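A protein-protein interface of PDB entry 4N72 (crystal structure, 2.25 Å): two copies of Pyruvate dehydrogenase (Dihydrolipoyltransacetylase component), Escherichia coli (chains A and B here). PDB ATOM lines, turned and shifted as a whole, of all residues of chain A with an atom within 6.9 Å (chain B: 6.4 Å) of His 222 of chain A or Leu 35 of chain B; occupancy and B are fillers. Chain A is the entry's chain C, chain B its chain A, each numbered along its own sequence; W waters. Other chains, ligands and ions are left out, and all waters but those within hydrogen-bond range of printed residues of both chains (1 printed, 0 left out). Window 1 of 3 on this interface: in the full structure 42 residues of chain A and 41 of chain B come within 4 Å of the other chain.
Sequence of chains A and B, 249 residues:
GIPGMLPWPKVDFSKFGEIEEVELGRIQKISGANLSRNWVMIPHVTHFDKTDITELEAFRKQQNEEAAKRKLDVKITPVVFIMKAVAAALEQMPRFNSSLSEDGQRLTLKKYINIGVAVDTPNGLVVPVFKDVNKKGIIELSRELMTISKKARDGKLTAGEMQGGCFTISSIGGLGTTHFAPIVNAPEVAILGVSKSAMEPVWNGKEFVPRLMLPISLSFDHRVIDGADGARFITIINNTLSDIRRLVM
The indole nitrogen of Trp 39 of chain B is in hydrogen-bond range of the backbone carbonyl oxygen of Ile 42 of chain A.
The backbone NH of Phe 220 of chain A sits at hydrogen-bond distance from the backbone carbonyl oxygen of Val 45 of chain A, at 2.9 Å. OD2 of Asp 221 of chain A lies within salt-bridge range of NH2 of Arg 223 of chain A (2.8 Å). ND1 of His 222 of chain A is in hydrogen-bond range of O of Ile 225 of chain A (2.7 Å). O of Pro 43 of chain A is in hydrogen-bond range of N of His 222 of chain A, at 3.0 Å. The backbone carbonyl oxygen of Ile 42 of chain A sits at hydrogen-bond distance from a ring nitrogen (ND1) of His 44 of chain A, at 2.6 Å. The backbone carbonyl oxygen of Gly 32 of chain B lies within hydrogen-bond range of the side-chain hydroxyl of Ser 36 of chain B, at 2.9 Å.
Leu 35 of chain B touches Pro 43 of chain A (O to CB, 3.99 Å). Trp 39 of chain B touches Pro 43 of chain A (CG to CA, 3.5 Å). Pro 43 of chain A touches Ile 183 of chain B. O of His 44 of chain A touches CZ3 of Trp 39 of chain B, 3.5 Å away. His 44 of chain A touches Ile 183 of chain B (O to CD1, 3.6 Å). Val 45 of chain A touches Ile 183 of chain B (CG2 to CG1, 3.9 Å). His 222 of chain A touches Leu 35 of chain B (O to CD1, 3.4 Å). Arg 223 of chain A touches Gly 32 of chain B. CD of Arg 223 of chain A touches OG of Ser 36 of chain B, at 3.7 Å.
Of chain B, only Leu 35 comes within 4 Å of His 222 of chain A. Of the printed residues of chain A, Gly 32 of chain B touches Arg 223 (3.9 Å). Printed residues of chain A within 4 Å of Leu 35 of chain B: Pro 43 and His 222. Printed residues of chain A within 4 Å of Ser 36 of chain B: Arg 223. Val 40 of chain B touches none of the printed residues of chain A. The nearest residue of chain B that does not touch His 222 of chain A is Ile 183 of chain B (4.1 Å).
Of the 14 printed residues of chain A, 6 touch a printed residue of chain B. Hydrophobic or aromatic side chains of chain A within 4 Å of the printed part of chain B: Pro 43, His 44, Val 45 and His 222. Of the 14 printed residues of chain B, 5 touch a printed residue of chain A. Hydrophobic or aromatic side chains of chain B that line the printed part of chain A: Leu 35, Trp 39 and Ile 183. Among the printed residues, no Asp or Glu carboxylate lies within 4 Å of a Lys or Arg side-chain nitrogen of the other chain.
No position is printed for both chains. Of the 10 pairs that touch across the chains among the printed residues, none has its exchanged pair printed and touching as well.
Water W1 bridges N of Ile 183 of chain B and NE2 of His 222 of chain A.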
ATOM      1  N   ILE A  42      -2.773  17.151   2.736  1.00  0.00           N
ATOM      2  CA  ILE A  42      -3.108  18.562   2.903  1.00  0.00           C
ATOM      3  C   ILE A  42      -4.470  18.760   3.565  1.00  0.00           C
ATOM      4  O   ILE A  42      -5.505  18.528   2.940  1.00  0.00           O
ATOM      5  CB  ILE A  42      -3.109  19.300   1.548  1.00  0.00           C
ATOM      6  CG1 ILE A  42      -1.750  19.159   0.858  1.00  0.00           C
ATOM      7  CG2 ILE A  42      -3.471  20.765   1.736  1.00  0.00           C
ATOM      8  CD1 ILE A  42      -1.682  19.831  -0.497  1.00  0.00           C
ATOM      9  N   PRO A  43      -4.475  19.188   4.838  1.00  0.00           N
ATOM     10  CA  PRO A  43      -5.743  19.519   5.496  1.00  0.00           C
ATOM     11  C   PRO A  43      -6.389  20.742   4.850  1.00  0.00           C
ATOM     12  O   PRO A  43      -5.918  21.867   5.030  1.00  0.00           O
ATOM     13  CB  PRO A  43      -5.329  19.815   6.942  1.00  0.00           C
ATOM     14  CG  PRO A  43      -3.879  20.137   6.874  1.00  0.00           C
ATOM     15  CD  PRO A  43      -3.327  19.314   5.752  1.00  0.00           C
ATOM     16  N   HIS A  44      -7.464  20.507   4.103  1.00  0.00           N
ATOM     17  CA  HIS A  44      -8.100  21.541   3.293  1.00  0.00           C
ATOM     18  C   HIS A  44      -9.100  22.404   4.056  1.00  0.00           C
ATOM     19  O   HIS A  44      -9.940  21.896   4.798  1.00  0.00           O
ATOM     20  CB  HIS A  44      -8.818  20.907   2.096  1.00  0.00           C
ATOM     21  CG  HIS A  44      -7.905  20.521   0.973  1.00  0.00           C
ATOM     22  ND1 HIS A  44      -6.984  19.499   1.080  1.00  0.00           N
ATOM     23  CD2 HIS A  44      -7.780  21.012  -0.279  1.00  0.00           C
ATOM     24  CE1 HIS A  44      -6.329  19.383  -0.060  1.00  0.00           C
ATOM     25  NE2 HIS A  44      -6.790  20.289  -0.903  1.00  0.00           N
ATOM     26  N   VAL A  45      -8.999  23.714   3.856  1.00  0.00           N
ATOM     27  CA  VAL A  45     -10.042  24.647   4.264  1.00  0.00           C
ATOM     28  C   VAL A  45     -10.432  25.471   3.042  1.00  0.00           C
ATOM     29  O   VAL A  45      -9.568  25.910   2.286  1.00  0.00           O
ATOM     30  CB  VAL A  45      -9.573  25.590   5.389  1.00  0.00           C
ATOM     31  CG1 VAL A  45     -10.618  26.671   5.652  1.00  0.00           C
ATOM     32  CG2 VAL A  45      -9.289  24.805   6.658  1.00  0.00           C
ATOM     33  N   VAL A 189       0.419  26.029  -2.129  1.00  0.00           N
ATOM     34  CA  VAL A 189      -0.307  26.078  -0.860  1.00  0.00           C
ATOM     35  C   VAL A 189      -1.759  26.559  -0.964  1.00  0.00           C
ATOM     36  O   VAL A 189      -2.513  26.456   0.003  1.00  0.00           O
ATOM     37  CB  VAL A 189       0.436  26.920   0.201  1.00  0.00           C
ATOM     38  CG1 VAL A 189       1.842  26.361   0.439  1.00  0.00           C
ATOM     39  CG2 VAL A 189       0.474  28.385  -0.203  1.00  0.00           C
ATOM     40  N   PHE A 220      -7.085  26.222   0.748  1.00  0.00           N
ATOM     41  CA  PHE A 220      -5.695  26.369   1.164  1.00  0.00           C
ATOM     42  C   PHE A 220      -5.221  25.307   2.152  1.00  0.00           C
ATOM     43  O   PHE A 220      -6.017  24.693   2.863  1.00  0.00           O
ATOM     44  CB  PHE A 220      -5.434  27.774   1.723  1.00  0.00           C
ATOM     45  CG  PHE A 220      -6.362  28.177   2.835  1.00  0.00           C
ATOM     46  CD1 PHE A 220      -6.087  27.835   4.150  1.00  0.00           C
ATOM     47  CD2 PHE A 220      -7.502  28.918   2.568  1.00  0.00           C
ATOM     48  CE1 PHE A 220      -6.937  28.213   5.173  1.00  0.00           C
ATOM     49  CE2 PHE A 220      -8.355  29.298   3.586  1.00  0.00           C
ATOM     50  CZ  PHE A 220      -8.071  28.946   4.890  1.00  0.00           C
ATOM     51  N   ASP A 221      -3.907  25.103   2.175  1.00  0.00           N
ATOM     52  CA  ASP A 221      -3.264  24.186   3.104  1.00  0.00           C
ATOM     53  C   ASP A 221      -3.310  24.787   4.506  1.00  0.00           C
ATOM     54  O   ASP A 221      -2.639  25.781   4.782  1.00  0.00           O
ATOM     55  CB  ASP A 221      -1.811  23.963   2.674  1.00  0.00           C
ATOM     56  CG  ASP A 221      -1.173  22.759   3.345  1.00  0.00           C
ATOM     57  OD1 ASP A 221      -1.645  22.346   4.425  1.00  0.00           O
ATOM     58  OD2 ASP A 221      -0.191  22.226   2.787  1.00  0.00           O
ATOM     59  N   HIS A 222      -4.096  24.180   5.392  1.00  0.00           N
ATOM     60  CA  HIS A 222      -4.296  24.731   6.730  1.00  0.00           C
ATOM     61  C   HIS A 222      -3.072  24.562   7.633  1.00  0.00           C
ATOM     62  O   HIS A 222      -3.016  25.129   8.725  1.00  0.00           O
ATOM     63  CB  HIS A 222      -5.538  24.129   7.394  1.00  0.00           C
ATOM     64  CG  HIS A 222      -6.067  24.947   8.531  1.00  0.00           C
ATOM     65  ND1 HIS A 222      -5.706  26.262   8.731  1.00  0.00           N
ATOM     66  CD2 HIS A 222      -6.927  24.637   9.531  1.00  0.00           C
ATOM     67  CE1 HIS A 222      -6.320  26.728   9.803  1.00  0.00           C
ATOM     68  NE2 HIS A 222      -7.068  25.762  10.306  1.00  0.00           N
ATOM     69  N   ARG A 223      -2.099  23.778   7.178  1.00  0.00           N
ATOM     70  CA  ARG A 223      -0.835  23.646   7.893  1.00  0.00           C
ATOM     71  C   ARG A 223      -0.059  24.951   7.806  1.00  0.00           C
ATOM     72  O   ARG A 223       0.645  25.334   8.740  1.00  0.00           O
ATOM     73  CB  ARG A 223       0.015  22.520   7.298  1.00  0.00           C
ATOM     74  CG  ARG A 223      -0.531  21.123   7.514  1.00  0.00           C
ATOM     75  CD  ARG A 223       0.351  20.085   6.836  1.00  0.00           C
ATOM     76  NE  ARG A 223       0.510  20.357   5.410  1.00  0.00           N
ATOM     77  CZ  ARG A 223       1.205  19.592   4.574  1.00  0.00           C
ATOM     78  NH1 ARG A 223       1.810  18.498   5.017  1.00  0.00           N
ATOM     79  NH2 ARG A 223       1.294  19.921   3.293  1.00  0.00           N
ATOM     80  N   VAL A 224      -0.202  25.631   6.672  1.00  0.00           N
ATOM     81  CA  VAL A 224       0.564  26.836   6.383  1.00  0.00           C
ATOM     82  C   VAL A 224      -0.249  28.099   6.646  1.00  0.00           C
ATOM     83  O   VAL A 224       0.245  29.059   7.240  1.00  0.00           O
ATOM     84  CB  VAL A 224       1.035  26.843   4.914  1.00  0.00           C
ATOM     85  CG1 VAL A 224       1.866  28.083   4.620  1.00  0.00           C
ATOM     86  CG2 VAL A 224       1.821  25.577   4.603  1.00  0.00           C
ATOM     87  N   ILE A 225      -1.502  28.088   6.202  1.00  0.00           N
ATOM     88  CA  ILE A 225      -2.372  29.254   6.308  1.00  0.00           C
ATOM     89  C   ILE A 225      -3.492  29.022   7.317  1.00  0.00           C
ATOM     90  O   ILE A 225      -4.152  27.984   7.286  1.00  0.00           O
ATOM     91  CB  ILE A 225      -3.022  29.575   4.949  1.00  0.00           C
ATOM     92  CG1 ILE A 225      -1.964  29.651   3.845  1.00  0.00           C
ATOM     93  CG2 ILE A 225      -3.828  30.861   5.036  1.00  0.00           C
ATOM     94  CD1 ILE A 225      -1.036  30.838   3.962  1.00  0.00           C
ATOM     95  N   ASP A 226      -3.709  29.985   8.209  1.00  0.00           N
ATOM     96  CA  ASP A 226      -4.841  29.905   9.129  1.00  0.00           C
ATOM     97  C   ASP A 226      -6.048  30.656   8.566  1.00  0.00           C
ATOM     98  O   ASP A 226      -5.915  31.444   7.629  1.00  0.00           O
ATOM     99  CB  ASP A 226      -4.475  30.413  10.529  1.00  0.00           C
ATOM    100  CG  ASP A 226      -4.161  31.894  10.555  1.00  0.00           C
ATOM    101  OD1 ASP A 226      -3.313  32.335   9.753  1.00  0.00           O
ATOM    102  OD2 ASP A 226      -4.765  32.617  11.376  1.00  0.00           O
ATOM    103  N   GLY A 227      -7.219  30.401   9.143  1.00  0.00           N
ATOM    104  CA  GLY A 227      -8.473  30.929   8.631  1.00  0.00           C
ATOM    105  C   GLY A 227      -8.539  32.437   8.481  1.00  0.00           C
ATOM    106  O   GLY A 227      -9.119  32.946   7.521  1.00  0.00           O
ATOM    107  N   ALA A 228      -7.949  33.153   9.433  1.00  0.00           N
ATOM    108  CA  ALA A 228      -7.934  34.610   9.397  1.00  0.00           C
ATOM    109  C   ALA A 228      -7.136  35.121   8.202  1.00  0.00           C
ATOM    110  O   ALA A 228      -7.563  36.044   7.507  1.00  0.00           O
ATOM    111  CB  ALA A 228      -7.363  35.164  10.693  1.00  0.00           C
ATOM    112  N   ILE B  30       3.197  22.148  15.863  1.00  0.00           N
ATOM    113  CA  ILE B  30       2.248  21.427  16.707  1.00  0.00           C
ATOM    114  C   ILE B  30       0.836  21.497  16.126  1.00  0.00           C
ATOM    115  O   ILE B  30       0.150  20.478  16.018  1.00  0.00           O
ATOM    116  CB  ILE B  30       2.263  21.953  18.166  1.00  0.00           C
ATOM    117  CG1 ILE B  30       3.282  21.182  19.010  1.00  0.00           C
ATOM    118  CG2 ILE B  30       0.890  21.821  18.812  1.00  0.00           C
ATOM    119  CD1 ILE B  30       4.727  21.445  18.647  1.00  0.00           C
ATOM    120  N   SER B  31       0.412  22.699  15.743  1.00  0.00           N
ATOM    121  CA  SER B  31      -0.927  22.902  15.200  1.00  0.00           C
ATOM    122  C   SER B  31      -1.114  22.164  13.879  1.00  0.00           C
ATOM    123  O   SER B  31      -2.107  21.464  13.690  1.00  0.00           O
ATOM    124  CB  SER B  31      -1.220  24.393  15.023  1.00  0.00           C
ATOM    125  OG  SER B  31      -0.255  25.009  14.189  1.00  0.00           O
ATOM    126  N   GLY B  32      -0.153  22.320  12.973  1.00  0.00           N
ATOM    127  CA  GLY B  32      -0.196  21.646  11.687  1.00  0.00           C
ATOM    128  C   GLY B  32      -0.178  20.137  11.832  1.00  0.00           C
ATOM    129  O   GLY B  32      -0.676  19.409  10.973  1.00  0.00           O
ATOM    130  N   ALA B  33       0.400  19.668  12.933  1.00  0.00           N
ATOM    131  CA  ALA B  33       0.448  18.245  13.232  1.00  0.00           C
ATOM    132  C   ALA B  33      -0.892  17.772  13.790  1.00  0.00           C
ATOM    133  O   ALA B  33      -1.347  16.668  13.488  1.00  0.00           O
ATOM    134  CB  ALA B  33       1.566  17.962  14.209  1.00  0.00           C
ATOM    135  N   ASN B  34      -1.514  18.614  14.611  1.00  0.00           N
ATOM    136  CA  ASN B  34      -2.862  18.360  15.101  1.00  0.00           C
ATOM    137  C   ASN B  34      -3.852  18.325  13.948  1.00  0.00           C
ATOM    138  O   ASN B  34      -4.726  17.461  13.886  1.00  0.00           O
ATOM    139  CB  ASN B  34      -3.288  19.449  16.090  1.00  0.00           C
ATOM    140  CG  ASN B  34      -2.708  19.247  17.475  1.00  0.00           C
ATOM    141  OD1 ASN B  34      -2.696  18.133  17.999  1.00  0.00           O
ATOM    142  ND2 ASN B  34      -2.230  20.327  18.079  1.00  0.00           N
ATOM    143  N   LEU B  35      -3.701  19.278  13.035  1.00  0.00           N
ATOM    144  CA  LEU B  35      -4.620  19.440  11.915  1.00  0.00           C
ATOM    145  C   LEU B  35      -4.560  18.273  10.935  1.00  0.00           C
ATOM    146  O   LEU B  35      -5.587  17.848  10.406  1.00  0.00           O
ATOM    147  CB  LEU B  35      -4.348  20.761  11.194  1.00  0.00           C
ATOM    148  CG  LEU B  35      -4.717  22.011  11.998  1.00  0.00           C
ATOM    149  CD1 LEU B  35      -4.080  23.257  11.398  1.00  0.00           C
ATOM    150  CD2 LEU B  35      -6.230  22.162  12.080  1.00  0.00           C
ATOM    151  N   SER B  36      -3.356  17.761  10.695  1.00  0.00           N
ATOM    152  CA  SER B  36      -3.176  16.611   9.816  1.00  0.00           C
ATOM    153  C   SER B  36      -3.902  15.392  10.373  1.00  0.00           C
ATOM    154  O   SER B  36      -4.548  14.651   9.633  1.00  0.00           O
ATOM    155  CB  SER B  36      -1.690  16.301   9.628  1.00  0.00           C
ATOM    156  OG  SER B  36      -1.030  17.363   8.963  1.00  0.00           O
ATOM    157  N   ARG B  37      -3.792  15.196  11.684  1.00  0.00           N
ATOM    158  CA  ARG B  37      -4.490  14.109  12.359  1.00  0.00           C
ATOM    159  C   ARG B  37      -6.001  14.307  12.283  1.00  0.00           C
ATOM    160  O   ARG B  37      -6.736  13.388  11.927  1.00  0.00           O
ATOM    161  CB  ARG B  37      -4.045  14.008  13.819  1.00  0.00           C
ATOM    162  CG  ARG B  37      -4.874  13.043  14.652  1.00  0.00           C
ATOM    163  CD  ARG B  37      -5.618  13.774  15.757  1.00  0.00           C
ATOM    164  NE  ARG B  37      -4.705  14.325  16.753  1.00  0.00           N
ATOM    165  CZ  ARG B  37      -4.903  15.471  17.397  1.00  0.00           C
ATOM    166  NH1 ARG B  37      -5.984  16.196  17.146  1.00  0.00           N
ATOM    167  NH2 ARG B  37      -4.018  15.894  18.289  1.00  0.00           N
ATOM    168  N   ASN B  38      -6.453  15.511  12.620  1.00  0.00           N
ATOM    169  CA  ASN B  38      -7.872  15.848  12.563  1.00  0.00           C
ATOM    170  C   ASN B  38      -8.462  15.643  11.172  1.00  0.00           C
ATOM    171  O   ASN B  38      -9.594  15.180  11.029  1.00  0.00           O
ATOM    172  CB  ASN B  38      -8.106  17.295  13.008  1.00  0.00           C
ATOM    173  CG  ASN B  38      -7.738  17.529  14.461  1.00  0.00           C
ATOM    174  OD1 ASN B  38      -7.523  16.585  15.218  1.00  0.00           O
ATOM    175  ND2 ASN B  38      -7.673  18.794  14.858  1.00  0.00           N
ATOM    176  N   TRP B  39      -7.684  15.984  10.151  1.00  0.00           N
ATOM    177  CA  TRP B  39      -8.151  15.932   8.769  1.00  0.00           C
ATOM    178  C   TRP B  39      -8.406  14.510   8.269  1.00  0.00           C
ATOM    179  O   TRP B  39      -9.370  14.270   7.542  1.00  0.00           O
ATOM    180  CB  TRP B  39      -7.159  16.654   7.849  1.00  0.00           C
ATOM    181  CG  TRP B  39      -7.508  16.585   6.390  1.00  0.00           C
ATOM    182  CD1 TRP B  39      -6.823  15.917   5.416  1.00  0.00           C
ATOM    183  CD2 TRP B  39      -8.625  17.207   5.743  1.00  0.00           C
ATOM    184  NE1 TRP B  39      -7.445  16.085   4.202  1.00  0.00           N
ATOM    185  CE2 TRP B  39      -8.553  16.872   4.375  1.00  0.00           C
ATOM    186  CE3 TRP B  39      -9.679  18.012   6.185  1.00  0.00           C
ATOM    187  CZ2 TRP B  39      -9.493  17.315   3.447  1.00  0.00           C
ATOM    188  CZ3 TRP B  39     -10.611  18.452   5.262  1.00  0.00           C
ATOM    189  CH2 TRP B  39     -10.512  18.102   3.909  1.00  0.00           C
ATOM    190  N   VAL B  40      -7.554  13.569   8.663  1.00  0.00           N
ATOM    191  CA  VAL B  40      -7.652  12.205   8.147  1.00  0.00           C
ATOM    192  C   VAL B  40      -8.497  11.274   9.020  1.00  0.00           C
ATOM    193  O   VAL B  40      -9.021  10.273   8.533  1.00  0.00           O
ATOM    194  CB  VAL B  40      -6.261  11.566   7.934  1.00  0.00           C
ATOM    195  CG1 VAL B  40      -5.368  12.486   7.114  1.00  0.00           C
ATOM    196  CG2 VAL B  40      -5.618  11.244   9.268  1.00  0.00           C
ATOM    197  N   ILE B 183     -12.214  22.974   9.749  1.00  0.00           N
ATOM    198  CA  ILE B 183     -11.882  21.620  10.176  1.00  0.00           C
ATOM    199  C   ILE B 183     -12.203  21.417  11.659  1.00  0.00           C
ATOM    200  O   ILE B 183     -11.905  22.275  12.490  1.00  0.00           O
ATOM    201  CB  ILE B 183     -10.389  21.315   9.923  1.00  0.00           C
ATOM    202  CG1 ILE B 183     -10.072  21.419   8.429  1.00  0.00           C
ATOM    203  CG2 ILE B 183     -10.012  19.939  10.455  1.00  0.00           C
ATOM    204  CD1 ILE B 183      -8.612  21.198   8.100  1.00  0.00           C
ATOM    205  N   VAL B 184     -12.818  20.282  11.977  1.00  0.00           N
ATOM    206  CA  VAL B 184     -13.188  19.954  13.352  1.00  0.00           C
ATOM    207  C   VAL B 184     -11.964  19.794  14.253  1.00  0.00           C
ATOM    208  O   VAL B 184     -10.991  19.132  13.886  1.00  0.00           O
ATOM    209  CB  VAL B 184     -14.031  18.662  13.407  1.00  0.00           C
ATOM    210  CG1 VAL B 184     -14.310  18.259  14.849  1.00  0.00           C
ATOM    211  CG2 VAL B 184     -15.331  18.841  12.637  1.00  0.00           C
ATOM    212  N   ASN B 185     -12.017  20.412  15.429  1.00  0.00           N
ATOM    213  CA  ASN B 185     -10.951  20.286  16.415  1.00  0.00           C
ATOM    214  C   ASN B 185     -11.159  19.100  17.348  1.00  0.00           C
ATOM    215  O   ASN B 185     -11.807  19.231  18.384  1.00  0.00           O
ATOM    216  CB  ASN B 185     -10.827  21.571  17.238  1.00  0.00           C
ATOM    217  CG  ASN B 185      -9.982  22.623  16.552  1.00  0.00           C
ATOM    218  OD1 ASN B 185     -10.482  23.676  16.153  1.00  0.00           O
ATOM    219  ND2 ASN B 185      -8.689  22.347  16.418  1.00  0.00           N
HETATM  220  O   HOH W   1     -10.368  25.343  10.137  1.00  0.00           O
